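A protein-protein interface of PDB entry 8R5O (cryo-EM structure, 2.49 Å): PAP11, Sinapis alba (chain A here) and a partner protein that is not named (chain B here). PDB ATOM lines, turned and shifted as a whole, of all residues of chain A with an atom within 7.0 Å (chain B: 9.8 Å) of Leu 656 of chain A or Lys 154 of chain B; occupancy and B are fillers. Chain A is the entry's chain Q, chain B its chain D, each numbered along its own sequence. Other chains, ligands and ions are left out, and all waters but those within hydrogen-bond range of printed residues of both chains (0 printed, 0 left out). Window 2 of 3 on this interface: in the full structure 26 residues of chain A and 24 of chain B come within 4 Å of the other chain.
OH of Tyr 682 of chain A lies within hydrogen-bond range of O of Thr 156 of chain B (3.4 Å). The guanidinium group of Arg 190 of chain B is in salt-bridge range of the side-chain carboxylate of Asp 695 of chain A.
CD1 of Leu 656 of chain A touches NZ of Lys 154 of chain B, 3.9 Å away. Leu 674 of chain A touches Thr 152 of chain B. Leu 674 of chain A touches Lys 153 of chain B (CD1 to O, 3.5 Å). Lys 154 of chain B touches Leu 674 of chain A. Leu 674 of chain A touches Pro 155 of chain B (CD2 to N, 3.95 Å). Pro 155 of chain B touches Leu 693 of chain A. O of Pro 155 of chain B touches NE2 of His 694 of chain A, at 3.7 Å. His 694 of chain A touches Phe 157 of chain B. CE1 of His 694 of chain A touches NH2 of Arg 190 of chain B, 3.99 Å away. Asp 695 of chain A touches Pro 155 of chain B.
Of the 17 printed residues of chain B, 7 touch a printed residue of chain A. Hydrophobic or aromatic side chains of chain B within 4 Å of the printed part of chain A: Pro 155 and Phe 157. Printed residues of chain A that touch a printed residue of chain B: Leu 656, Leu 674, Tyr 682, Leu 693, His 694 and Asp 695. Hydrophobic or aromatic side chains of chain A within 4 Å of the printed part of chain B: Leu 656, Leu 674, Tyr 682, Leu 693 and His 694.
N of Leu 656 of chain A sits close to OD2 of Asp 654 of chain A (3.3 Å). The side-chain hydroxyl (OH) of Tyr 673 of chain A lies within hydrogen-bond range of the backbone NH (N) of Leu 693 of chain A (2.9 Å). The backbone NH of Phe 157 of chain B sits at hydrogen-bond distance from the side-chain carboxylate of Glu 191 of chain B, at 3.3 Å. The guanidinium group of Arg 190 of chain B sits at hydrogen-bond distance from the backbone carbonyl oxygen of Pro 155 of chain B (2.9 Å). The side-chain hydroxyl (OG) of Ser 647 of chain A sits at hydrogen-bond distance from the backbone carbonyl oxygen (O) of Asp 695 of chain A.
Of the printed residues of chain B, Leu 656 of chain A touches Lys 154 (3.9 Å). Lys 154 of chain B touches two residues of chain A. No residue of chain B comes within 4 Å of Asp 654 of chain A. No residue of chain B comes within 4 Å of Pro 655 of chain A. No residue of chain B comes within 4 Å of Asp 657 of chain A. Of the printed residues of chain A, Thr 152 of chain B touches Leu 674 (3.9 Å). Printed residues of chain B within 4 Å of Tyr 682 of chain A: Thr 156 (3.4 Å). Printed residues of chain A within 4 Å of Arg 190 of chain B: His 694 and Asp 695. The nearest residue of chain A that does not touch Lys 154 of chain B is Asp 695 of chain A (4.7 Å).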
ATOM      1  N   SER A 647      30.230 -15.040  11.033  1.00  0.00           N
ATOM      2  CA  SER A 647      30.737 -14.024  10.123  1.00  0.00           C
ATOM      3  C   SER A 647      31.248 -14.681   8.849  1.00  0.00           C
ATOM      4  O   SER A 647      32.063 -15.607   8.908  1.00  0.00           O
ATOM      5  CB  SER A 647      31.856 -13.219  10.785  1.00  0.00           C
ATOM      6  OG  SER A 647      31.451 -12.731  12.051  1.00  0.00           O
ATOM      7  N   GLU A 653      33.063  -3.686   7.966  1.00  0.00           N
ATOM      8  CA  GLU A 653      31.912  -3.591   8.848  1.00  0.00           C
ATOM      9  C   GLU A 653      32.111  -4.479  10.071  1.00  0.00           C
ATOM     10  O   GLU A 653      32.716  -5.552   9.993  1.00  0.00           O
ATOM     11  CB  GLU A 653      30.631  -3.986   8.111  1.00  0.00           C
ATOM     12  CG  GLU A 653      29.352  -3.684   8.871  1.00  0.00           C
ATOM     13  CD  GLU A 653      28.113  -3.862   8.017  1.00  0.00           C
ATOM     14  OE1 GLU A 653      28.257  -4.233   6.834  1.00  0.00           O
ATOM     15  OE2 GLU A 653      26.997  -3.629   8.526  1.00  0.00           O
ATOM     16  N   ASP A 654      31.602  -4.016  11.205  1.00  0.00           N
ATOM     17  CA  ASP A 654      31.741  -4.767  12.445  1.00  0.00           C
ATOM     18  C   ASP A 654      30.904  -6.040  12.378  1.00  0.00           C
ATOM     19  O   ASP A 654      29.727  -5.981  12.002  1.00  0.00           O
ATOM     20  CB  ASP A 654      31.318  -3.909  13.635  1.00  0.00           C
ATOM     21  CG  ASP A 654      31.513  -4.614  14.962  1.00  0.00           C
ATOM     22  OD1 ASP A 654      32.676  -4.880  15.332  1.00  0.00           O
ATOM     23  OD2 ASP A 654      30.503  -4.900  15.638  1.00  0.00           O
ATOM     24  N   PRO A 655      31.469  -7.202  12.717  1.00  0.00           N
ATOM     25  CA  PRO A 655      30.702  -8.453  12.599  1.00  0.00           C
ATOM     26  C   PRO A 655      29.451  -8.496  13.457  1.00  0.00           C
ATOM     27  O   PRO A 655      28.467  -9.132  13.061  1.00  0.00           O
ATOM     28  CB  PRO A 655      31.718  -9.524  13.022  1.00  0.00           C
ATOM     29  CG  PRO A 655      32.734  -8.795  13.827  1.00  0.00           C
ATOM     30  CD  PRO A 655      32.833  -7.433  13.219  1.00  0.00           C
ATOM     31  N   LEU A 656      29.449  -7.845  14.621  1.00  0.00           N
ATOM     32  CA  LEU A 656      28.264  -7.863  15.469  1.00  0.00           C
ATOM     33  C   LEU A 656      27.144  -6.989  14.920  1.00  0.00           C
ATOM     34  O   LEU A 656      25.985  -7.182  15.299  1.00  0.00           O
ATOM     35  CB  LEU A 656      28.622  -7.426  16.891  1.00  0.00           C
ATOM     36  CG  LEU A 656      29.546  -8.361  17.672  1.00  0.00           C
ATOM     37  CD1 LEU A 656      29.694  -7.891  19.109  1.00  0.00           C
ATOM     38  CD2 LEU A 656      29.031  -9.788  17.622  1.00  0.00           C
ATOM     39  N   ASP A 657      27.462  -6.033  14.044  1.00  0.00           N
ATOM     40  CA  ASP A 657      26.423  -5.240  13.399  1.00  0.00           C
ATOM     41  C   ASP A 657      25.709  -6.037  12.316  1.00  0.00           C
ATOM     42  O   ASP A 657      24.489  -5.921  12.156  1.00  0.00           O
ATOM     43  CB  ASP A 657      27.020  -3.962  12.814  1.00  0.00           C
ATOM     44  CG  ASP A 657      27.415  -2.962  13.880  1.00  0.00           C
ATOM     45  OD1 ASP A 657      28.337  -3.261  14.665  1.00  0.00           O
ATOM     46  OD2 ASP A 657      26.803  -1.875  13.934  1.00  0.00           O
ATOM     47  N   ILE A 658      26.454  -6.848  11.563  1.00  0.00           N
ATOM     48  CA  ILE A 658      25.836  -7.722  10.571  1.00  0.00           C
ATOM     49  C   ILE A 658      24.948  -8.752  11.254  1.00  0.00           C
ATOM     50  O   ILE A 658      23.829  -9.026  10.805  1.00  0.00           O
ATOM     51  CB  ILE A 658      26.918  -8.394   9.707  1.00  0.00           C
ATOM     52  CG1 ILE A 658      27.882  -7.345   9.158  1.00  0.00           C
ATOM     53  CG2 ILE A 658      26.281  -9.182   8.574  1.00  0.00           C
ATOM     54  CD1 ILE A 658      29.069  -7.931   8.449  1.00  0.00           C
ATOM     55  N   LEU A 659      25.433  -9.341  12.350  1.00  0.00           N
ATOM     56  CA  LEU A 659      24.641 -10.327  13.077  1.00  0.00           C
ATOM     57  C   LEU A 659      23.390  -9.708  13.681  1.00  0.00           C
ATOM     58  O   LEU A 659      22.373 -10.392  13.834  1.00  0.00           O
ATOM     59  CB  LEU A 659      25.489 -10.985  14.163  1.00  0.00           C
ATOM     60  CG  LEU A 659      26.615 -11.900  13.680  1.00  0.00           C
ATOM     61  CD1 LEU A 659      27.486 -12.354  14.840  1.00  0.00           C
ATOM     62  CD2 LEU A 659      26.036 -13.093  12.948  1.00  0.00           C
ATOM     63  N   ASP A 660      23.444  -8.424  14.040  1.00  0.00           N
ATOM     64  CA  ASP A 660      22.244  -7.741  14.511  1.00  0.00           C
ATOM     65  C   ASP A 660      21.213  -7.613  13.398  1.00  0.00           C
ATOM     66  O   ASP A 660      20.010  -7.771  13.636  1.00  0.00           O
ATOM     67  CB  ASP A 660      22.607  -6.367  15.071  1.00  0.00           C
ATOM     68  CG  ASP A 660      21.408  -5.636  15.641  1.00  0.00           C
ATOM     69  OD1 ASP A 660      20.906  -6.054  16.704  1.00  0.00           O
ATOM     70  OD2 ASP A 660      20.964  -4.647  15.021  1.00  0.00           O
ATOM     71  N   ASP A 661      21.664  -7.321  12.175  1.00  0.00           N
ATOM     72  CA  ASP A 661      20.750  -7.280  11.038  1.00  0.00           C
ATOM     73  C   ASP A 661      20.152  -8.652  10.765  1.00  0.00           C
ATOM     74  O   ASP A 661      18.963  -8.767  10.446  1.00  0.00           O
ATOM     75  CB  ASP A 661      21.472  -6.754   9.798  1.00  0.00           C
ATOM     76  CG  ASP A 661      21.831  -5.289   9.909  1.00  0.00           C
ATOM     77  OD1 ASP A 661      21.105  -4.551  10.606  1.00  0.00           O
ATOM     78  OD2 ASP A 661      22.836  -4.874   9.299  1.00  0.00           O
ATOM     79  N   LEU A 663      19.727 -11.050  13.027  1.00  0.00           N
ATOM     80  CA  LEU A 663      18.822 -11.373  14.126  1.00  0.00           C
ATOM     81  C   LEU A 663      17.471 -10.688  13.970  1.00  0.00           C
ATOM     82  O   LEU A 663      16.459 -11.195  14.467  1.00  0.00           O
ATOM     83  CB  LEU A 663      19.456 -10.985  15.462  1.00  0.00           C
ATOM     84  CG  LEU A 663      20.522 -11.923  16.025  1.00  0.00           C
ATOM     85  CD1 LEU A 663      21.146 -11.331  17.275  1.00  0.00           C
ATOM     86  CD2 LEU A 663      19.920 -13.285  16.319  1.00  0.00           C
ATOM     87  N   MET A 670      20.955  -8.225  19.198  1.00  0.00           N
ATOM     88  CA  MET A 670      22.189  -8.687  19.822  1.00  0.00           C
ATOM     89  C   MET A 670      22.147  -8.494  21.332  1.00  0.00           C
ATOM     90  O   MET A 670      22.648  -9.334  22.087  1.00  0.00           O
ATOM     91  CB  MET A 670      23.389  -7.958  19.220  1.00  0.00           C
ATOM     92  CG  MET A 670      24.723  -8.387  19.801  1.00  0.00           C
ATOM     93  SD  MET A 670      25.064 -10.140  19.556  1.00  0.00           S
ATOM     94  CE  MET A 670      25.192 -10.212  17.774  1.00  0.00           C
ATOM     95  N   TYR A 673      20.144 -11.318  22.894  1.00  0.00           N
ATOM     96  CA  TYR A 673      20.912 -12.559  22.867  1.00  0.00           C
ATOM     97  C   TYR A 673      22.010 -12.550  23.924  1.00  0.00           C
ATOM     98  O   TYR A 673      22.248 -13.563  24.591  1.00  0.00           O
ATOM     99  CB  TYR A 673      21.509 -12.784  21.478  1.00  0.00           C
ATOM    100  CG  TYR A 673      22.335 -14.045  21.375  1.00  0.00           C
ATOM    101  CD1 TYR A 673      21.735 -15.272  21.126  1.00  0.00           C
ATOM    102  CD2 TYR A 673      23.713 -14.012  21.531  1.00  0.00           C
ATOM    103  CE1 TYR A 673      22.483 -16.427  21.035  1.00  0.00           C
ATOM    104  CE2 TYR A 673      24.468 -15.162  21.443  1.00  0.00           C
ATOM    105  CZ  TYR A 673      23.850 -16.366  21.195  1.00  0.00           C
ATOM    106  OH  TYR A 673      24.603 -17.511  21.105  1.00  0.00           O
ATOM    107  N   LEU A 674      22.693 -11.416  24.087  1.00  0.00           N
ATOM    108  CA  LEU A 674      23.749 -11.328  25.088  1.00  0.00           C
ATOM    109  C   LEU A 674      23.189 -11.389  26.503  1.00  0.00           C
ATOM    110  O   LEU A 674      23.864 -11.884  27.412  1.00  0.00           O
ATOM    111  CB  LEU A 674      24.560 -10.051  24.885  1.00  0.00           C
ATOM    112  CG  LEU A 674      25.376  -9.988  23.594  1.00  0.00           C
ATOM    113  CD1 LEU A 674      26.094  -8.656  23.472  1.00  0.00           C
ATOM    114  CD2 LEU A 674      26.361 -11.140  23.529  1.00  0.00           C
ATOM    115  N   TYR A 682      19.982 -19.993  26.483  1.00  0.00           N
ATOM    116  CA  TYR A 682      19.388 -19.413  25.292  1.00  0.00           C
ATOM    117  C   TYR A 682      18.090 -20.135  24.981  1.00  0.00           C
ATOM    118  O   TYR A 682      18.122 -21.338  24.676  1.00  0.00           O
ATOM    119  CB  TYR A 682      20.345 -19.513  24.112  1.00  0.00           C
ATOM    120  CG  TYR A 682      21.694 -18.888  24.374  1.00  0.00           C
ATOM    121  CD1 TYR A 682      21.877 -17.518  24.275  1.00  0.00           C
ATOM    122  CD2 TYR A 682      22.786 -19.670  24.720  1.00  0.00           C
ATOM    123  CE1 TYR A 682      23.106 -16.943  24.513  1.00  0.00           C
ATOM    124  CE2 TYR A 682      24.020 -19.102  24.959  1.00  0.00           C
ATOM    125  CZ  TYR A 682      24.174 -17.739  24.854  1.00  0.00           C
ATOM    126  OH  TYR A 682      25.403 -17.171  25.092  1.00  0.00           O
ATOM    127  N   LEU A 693      24.975 -18.232  18.290  1.00  0.00           N
ATOM    128  CA  LEU A 693      25.644 -17.118  17.640  1.00  0.00           C
ATOM    129  C   LEU A 693      27.081 -17.020  18.130  1.00  0.00           C
ATOM    130  O   LEU A 693      27.357 -17.240  19.311  1.00  0.00           O
ATOM    131  CB  LEU A 693      24.881 -15.815  17.914  1.00  0.00           C
ATOM    132  CG  LEU A 693      25.297 -14.507  17.248  1.00  0.00           C
ATOM    133  CD1 LEU A 693      24.066 -13.663  16.999  1.00  0.00           C
ATOM    134  CD2 LEU A 693      26.279 -13.752  18.120  1.00  0.00           C
ATOM    135  N   HIS A 694      27.987 -16.697  17.207  1.00  0.00           N
ATOM    136  CA  HIS A 694      29.368 -16.380  17.546  1.00  0.00           C
ATOM    137  C   HIS A 694      30.005 -15.697  16.346  1.00  0.00           C
ATOM    138  O   HIS A 694      29.883 -16.187  15.220  1.00  0.00           O
ATOM    139  CB  HIS A 694      30.162 -17.631  17.936  1.00  0.00           C
ATOM    140  CG  HIS A 694      31.309 -17.348  18.855  1.00  0.00           C
ATOM    141  ND1 HIS A 694      32.504 -16.822  18.416  1.00  0.00           N
ATOM    142  CD2 HIS A 694      31.438 -17.507  20.193  1.00  0.00           C
ATOM    143  CE1 HIS A 694      33.322 -16.675  19.442  1.00  0.00           C
ATOM    144  NE2 HIS A 694      32.699 -17.083  20.532  1.00  0.00           N
ATOM    145  N   ASP A 695      30.685 -14.578  16.587  1.00  0.00           N
ATOM    146  CA  ASP A 695      31.211 -13.762  15.503  1.00  0.00           C
ATOM    147  C   ASP A 695      32.511 -14.296  14.917  1.00  0.00           C
ATOM    148  O   ASP A 695      32.936 -13.813  13.862  1.00  0.00           O
ATOM    149  CB  ASP A 695      31.420 -12.323  15.984  1.00  0.00           C
ATOM    150  CG  ASP A 695      32.198 -12.248  17.279  1.00  0.00           C
ATOM    151  OD1 ASP A 695      31.945 -13.078  18.175  1.00  0.00           O
ATOM    152  OD2 ASP A 695      33.068 -11.363  17.401  1.00  0.00           O
ATOM    153  N   ARG B 149      34.303 -15.385  32.511  1.00  0.00           N
ATOM    154  CA  ARG B 149      33.320 -14.477  31.930  1.00  0.00           C
ATOM    155  C   ARG B 149      33.567 -13.025  32.350  1.00  0.00           C
ATOM    156  O   ARG B 149      32.700 -12.394  32.963  1.00  0.00           O
ATOM    157  CB  ARG B 149      31.906 -14.909  32.295  1.00  0.00           C
ATOM    158  CG  ARG B 149      30.829 -14.380  31.361  1.00  0.00           C
ATOM    159  CD  ARG B 149      30.703 -15.243  30.119  1.00  0.00           C
ATOM    160  NE  ARG B 149      30.215 -16.579  30.439  1.00  0.00           N
ATOM    161  CZ  ARG B 149      28.933 -16.909  30.512  1.00  0.00           C
ATOM    162  NH1 ARG B 149      27.978 -16.024  30.278  1.00  0.00           N
ATOM    163  NH2 ARG B 149      28.600 -18.157  30.830  1.00  0.00           N
ATOM    164  N   PRO B 150      34.743 -12.468  32.044  1.00  0.00           N
ATOM    165  CA  PRO B 150      35.001 -11.076  32.440  1.00  0.00           C
ATOM    166  C   PRO B 150      34.130 -10.070  31.710  1.00  0.00           C
ATOM    167  O   PRO B 150      33.876  -8.985  32.246  1.00  0.00           O
ATOM    168  CB  PRO B 150      36.485 -10.890  32.099  1.00  0.00           C
ATOM    169  CG  PRO B 150      36.713 -11.822  30.970  1.00  0.00           C
ATOM    170  CD  PRO B 150      35.844 -13.020  31.236  1.00  0.00           C
ATOM    171  N   ILE B 151      33.661 -10.394  30.507  1.00  0.00           N
ATOM    172  CA  ILE B 151      32.925  -9.454  29.675  1.00  0.00           C
ATOM    173  C   ILE B 151      31.524  -9.998  29.428  1.00  0.00           C
ATOM    174  O   ILE B 151      31.250 -11.189  29.594  1.00  0.00           O
ATOM    175  CB  ILE B 151      33.642  -9.179  28.340  1.00  0.00           C
ATOM    176  CG1 ILE B 151      33.406 -10.323  27.358  1.00  0.00           C
ATOM    177  CG2 ILE B 151      35.133  -9.007  28.566  1.00  0.00           C
ATOM    178  CD1 ILE B 151      34.087 -10.120  26.030  1.00  0.00           C
ATOM    179  N   THR B 152      30.625  -9.096  29.030  1.00  0.00           N
ATOM    180  CA  THR B 152      29.245  -9.457  28.745  1.00  0.00           C
ATOM    181  C   THR B 152      28.710  -8.852  27.455  1.00  0.00           C
ATOM    182  O   THR B 152      27.531  -9.048  27.146  1.00  0.00           O
ATOM    183  CB  THR B 152      28.328  -9.040  29.905  1.00  0.00           C
ATOM    184  OG1 THR B 152      28.596  -7.679  30.264  1.00  0.00           O
ATOM    185  CG2 THR B 152      28.546  -9.935  31.114  1.00  0.00           C
ATOM    186  N   LYS B 153      29.531  -8.125  26.698  1.00  0.00           N
ATOM    187  CA  LYS B 153      29.096  -7.482  25.467  1.00  0.00           C
ATOM    188  C   LYS B 153      29.549  -8.223  24.215  1.00  0.00           C
ATOM    189  O   LYS B 153      29.411  -7.690  23.111  1.00  0.00           O
ATOM    190  CB  LYS B 153      29.595  -6.036  25.421  1.00  0.00           C
ATOM    191  CG  LYS B 153      29.047  -5.156  26.529  1.00  0.00           C
ATOM    192  CD  LYS B 153      29.475  -3.711  26.348  1.00  0.00           C
ATOM    193  CE  LYS B 153      29.064  -2.865  27.540  1.00  0.00           C
ATOM    194  NZ  LYS B 153      27.606  -2.967  27.819  1.00  0.00           N
ATOM    195  N   LYS B 154      30.083  -9.430  24.357  1.00  0.00           N
ATOM    196  CA  LYS B 154      30.521 -10.225  23.221  1.00  0.00           C
ATOM    197  C   LYS B 154      30.093 -11.669  23.422  1.00  0.00           C
ATOM    198  O   LYS B 154      29.915 -12.113  24.563  1.00  0.00           O
ATOM    199  CB  LYS B 154      32.044 -10.147  23.030  1.00  0.00           C
ATOM    200  CG  LYS B 154      32.512  -8.822  22.459  1.00  0.00           C
ATOM    201  CD  LYS B 154      33.958  -8.889  22.008  1.00  0.00           C
ATOM    202  CE  LYS B 154      34.336  -7.651  21.214  1.00  0.00           C
ATOM    203  NZ  LYS B 154      33.453  -7.464  20.031  1.00  0.00           N
ATOM    204  N   PRO B 155      29.903 -12.420  22.336  1.00  0.00           N
ATOM    205  CA  PRO B 155      29.421 -13.800  22.470  1.00  0.00           C
ATOM    206  C   PRO B 155      30.402 -14.690  23.216  1.00  0.00           C
ATOM    207  O   PRO B 155      31.620 -14.585  23.056  1.00  0.00           O
ATOM    208  CB  PRO B 155      29.254 -14.258  21.016  1.00  0.00           C
ATOM    209  CG  PRO B 155      29.093 -13.000  20.241  1.00  0.00           C
ATOM    210  CD  PRO B 155      29.955 -11.991  20.929  1.00  0.00           C
ATOM    211  N   THR B 156      29.848 -15.582  24.036  1.00  0.00           N
ATOM    212  CA  THR B 156      30.607 -16.596  24.753  1.00  0.00           C
ATOM    213  C   THR B 156      29.841 -17.908  24.682  1.00  0.00           C
ATOM    214  O   THR B 156      28.628 -17.927  24.459  1.00  0.00           O
ATOM    215  CB  THR B 156      30.858 -16.204  26.217  1.00  0.00           C
ATOM    216  OG1 THR B 156      29.619 -15.837  26.835  1.00  0.00           O
ATOM    217  CG2 THR B 156      31.832 -15.037  26.308  1.00  0.00           C
ATOM    218  N   PHE B 157      30.559 -19.019  24.876  1.00  0.00           N
ATOM    219  CA  PHE B 157      29.925 -20.326  24.735  1.00  0.00           C
ATOM    220  C   PHE B 157      30.318 -21.308  25.837  1.00  0.00           C
ATOM    221  O   PHE B 157      30.106 -22.515  25.678  1.00  0.00           O
ATOM    222  CB  PHE B 157      30.242 -20.935  23.363  1.00  0.00           C
ATOM    223  CG  PHE B 157      31.701 -21.204  23.137  1.00  0.00           C
ATOM    224  CD1 PHE B 157      32.550 -20.191  22.727  1.00  0.00           C
ATOM    225  CD2 PHE B 157      32.219 -22.473  23.317  1.00  0.00           C
ATOM    226  CE1 PHE B 157      33.890 -20.436  22.515  1.00  0.00           C
ATOM    227  CE2 PHE B 157      33.559 -22.724  23.106  1.00  0.00           C
ATOM    228  CZ  PHE B 157      34.394 -21.706  22.704  1.00  0.00           C
ATOM    229  N   LEU B 158      30.878 -20.831  26.944  1.00  0.00           N
ATOM    230  CA  LEU B 158      31.217 -21.678  28.076  1.00  0.00           C
ATOM    231  C   LEU B 158      30.398 -21.262  29.290  1.00  0.00           C
ATOM    232  O   LEU B 158      30.122 -20.076  29.492  1.00  0.00           O
ATOM    233  CB  LEU B 158      32.712 -21.602  28.399  1.00  0.00           C
ATOM    234  CG  LEU B 158      33.664 -21.948  27.252  1.00  0.00           C
ATOM    235  CD1 LEU B 158      35.107 -21.847  27.711  1.00  0.00           C
ATOM    236  CD2 LEU B 158      33.371 -23.333  26.703  1.00  0.00           C
ATOM    237  N   ILE B 186      42.417 -15.783  19.995  1.00  0.00           N
ATOM    238  CA  ILE B 186      41.537 -14.681  19.616  1.00  0.00           C
ATOM    239  C   ILE B 186      40.434 -14.495  20.651  1.00  0.00           C
ATOM    240  O   ILE B 186      40.175 -13.378  21.113  1.00  0.00           O
ATOM    241  CB  ILE B 186      40.958 -14.915  18.210  1.00  0.00           C
ATOM    242  CG1 ILE B 186      42.083 -14.983  17.177  1.00  0.00           C
ATOM    243  CG2 ILE B 186      39.969 -13.819  17.852  1.00  0.00           C
ATOM    244  CD1 ILE B 186      41.598 -15.188  15.760  1.00  0.00           C
ATOM    245  N   PHE B 187      39.773 -15.584  21.035  1.00  0.00           N
ATOM    246  CA  PHE B 187      38.653 -15.532  21.963  1.00  0.00           C
ATOM    247  C   PHE B 187      39.013 -16.029  23.357  1.00  0.00           C
ATOM    248  O   PHE B 187      38.116 -16.225  24.183  1.00  0.00           O
ATOM    249  CB  PHE B 187      37.471 -16.335  21.411  1.00  0.00           C
ATOM    250  CG  PHE B 187      37.699 -17.821  21.392  1.00  0.00           C
ATOM    251  CD1 PHE B 187      38.414 -18.414  20.365  1.00  0.00           C
ATOM    252  CD2 PHE B 187      37.187 -18.628  22.394  1.00  0.00           C
ATOM    253  CE1 PHE B 187      38.621 -19.777  20.344  1.00  0.00           C
ATOM    254  CE2 PHE B 187      37.393 -19.992  22.378  1.00  0.00           C
ATOM    255  CZ  PHE B 187      38.109 -20.568  21.352  1.00  0.00           C
ATOM    256  N   ASN B 189      40.701 -14.499  25.880  1.00  0.00           N
ATOM    257  CA  ASN B 189      40.430 -13.487  26.902  1.00  0.00           C
ATOM    258  C   ASN B 189      39.026 -12.912  26.755  1.00  0.00           C
ATOM    259  O   ASN B 189      38.800 -11.704  26.817  1.00  0.00           O
ATOM    260  CB  ASN B 189      41.485 -12.390  26.838  1.00  0.00           C
ATOM    261  CG  ASN B 189      42.881 -12.910  27.111  1.00  0.00           C
ATOM    262  OD1 ASN B 189      43.065 -13.881  27.846  1.00  0.00           O
ATOM    263  ND2 ASN B 189      43.878 -12.263  26.518  1.00  0.00           N
ATOM    264  N   ARG B 190      38.066 -13.814  26.568  1.00  0.00           N
ATOM    265  CA  ARG B 190      36.645 -13.492  26.601  1.00  0.00           C
ATOM    266  C   ARG B 190      35.831 -14.467  27.433  1.00  0.00           C
ATOM    267  O   ARG B 190      34.735 -14.105  27.870  1.00  0.00           O
ATOM    268  CB  ARG B 190      36.069 -13.446  25.181  1.00  0.00           C
ATOM    269  CG  ARG B 190      36.540 -12.254  24.370  1.00  0.00           C
ATOM    270  CD  ARG B 190      36.303 -12.448  22.883  1.00  0.00           C
ATOM    271  NE  ARG B 190      34.913 -12.749  22.567  1.00  0.00           N
ATOM    272  CZ  ARG B 190      34.417 -12.777  21.338  1.00  0.00           C
ATOM    273  NH1 ARG B 190      35.168 -12.506  20.284  1.00  0.00           N
ATOM    274  NH2 ARG B 190      33.135 -13.080  21.162  1.00  0.00           N
ATOM    275  N   GLU B 191      36.322 -15.681  27.673  1.00  0.00           N
ATOM    276  CA  GLU B 191      35.673 -16.662  28.532  1.00  0.00           C
ATOM    277  C   GLU B 191      36.220 -16.648  29.951  1.00  0.00           C
ATOM    278  O   GLU B 191      35.449 -16.736  30.910  1.00  0.00           O
ATOM    279  CB  GLU B 191      35.834 -18.066  27.944  1.00  0.00           C
ATOM    280  CG  GLU B 191      35.536 -18.157  26.459  1.00  0.00           C
ATOM    281  CD  GLU B 191      34.056 -18.098  26.153  1.00  0.00           C
ATOM    282  OE1 GLU B 191      33.245 -18.267  27.086  1.00  0.00           O
ATOM    283  OE2 GLU B 191      33.703 -17.885  24.976  1.00  0.00           O
ATOM    284  N   GLU B 201      38.913  -5.153  31.954  1.00  0.00           N
ATOM    285  CA  GLU B 201      37.828  -5.552  31.062  1.00  0.00           C
ATOM    286  C   GLU B 201      36.478  -5.454  31.760  1.00  0.00           C
ATOM    287  O   GLU B 201      35.487  -5.040  31.149  1.00  0.00           O
ATOM    288  CB  GLU B 201      38.062  -6.969  30.541  1.00  0.00           C
ATOM    289  CG  GLU B 201      39.412  -7.174  29.881  1.00  0.00           C
ATOM    290  CD  GLU B 201      39.679  -6.188  28.761  1.00  0.00           C
ATOM    291  OE1 GLU B 201      38.730  -5.848  28.023  1.00  0.00           O
ATOM    292  OE2 GLU B 201      40.840  -5.752  28.621  1.00  0.00           O
ATOM    293  N   ASP B 205      33.579  -2.724  30.571  1.00  0.00           N
ATOM    294  CA  ASP B 205      32.307  -3.269  30.115  1.00  0.00           C
ATOM    295  C   ASP B 205      31.161  -3.001  31.078  1.00  0.00           C
ATOM    296  O   ASP B 205      30.051  -3.489  30.846  1.00  0.00           O
ATOM    297  CB  ASP B 205      32.436  -4.777  29.876  1.00  0.00           C
ATOM    298  CG  ASP B 205      33.303  -5.103  28.678  1.00  0.00           C
ATOM    299  OD1 ASP B 205      33.111  -4.480  27.614  1.00  0.00           O
ATOM    300  OD2 ASP B 205      34.184  -5.977  28.803  1.00  0.00           O
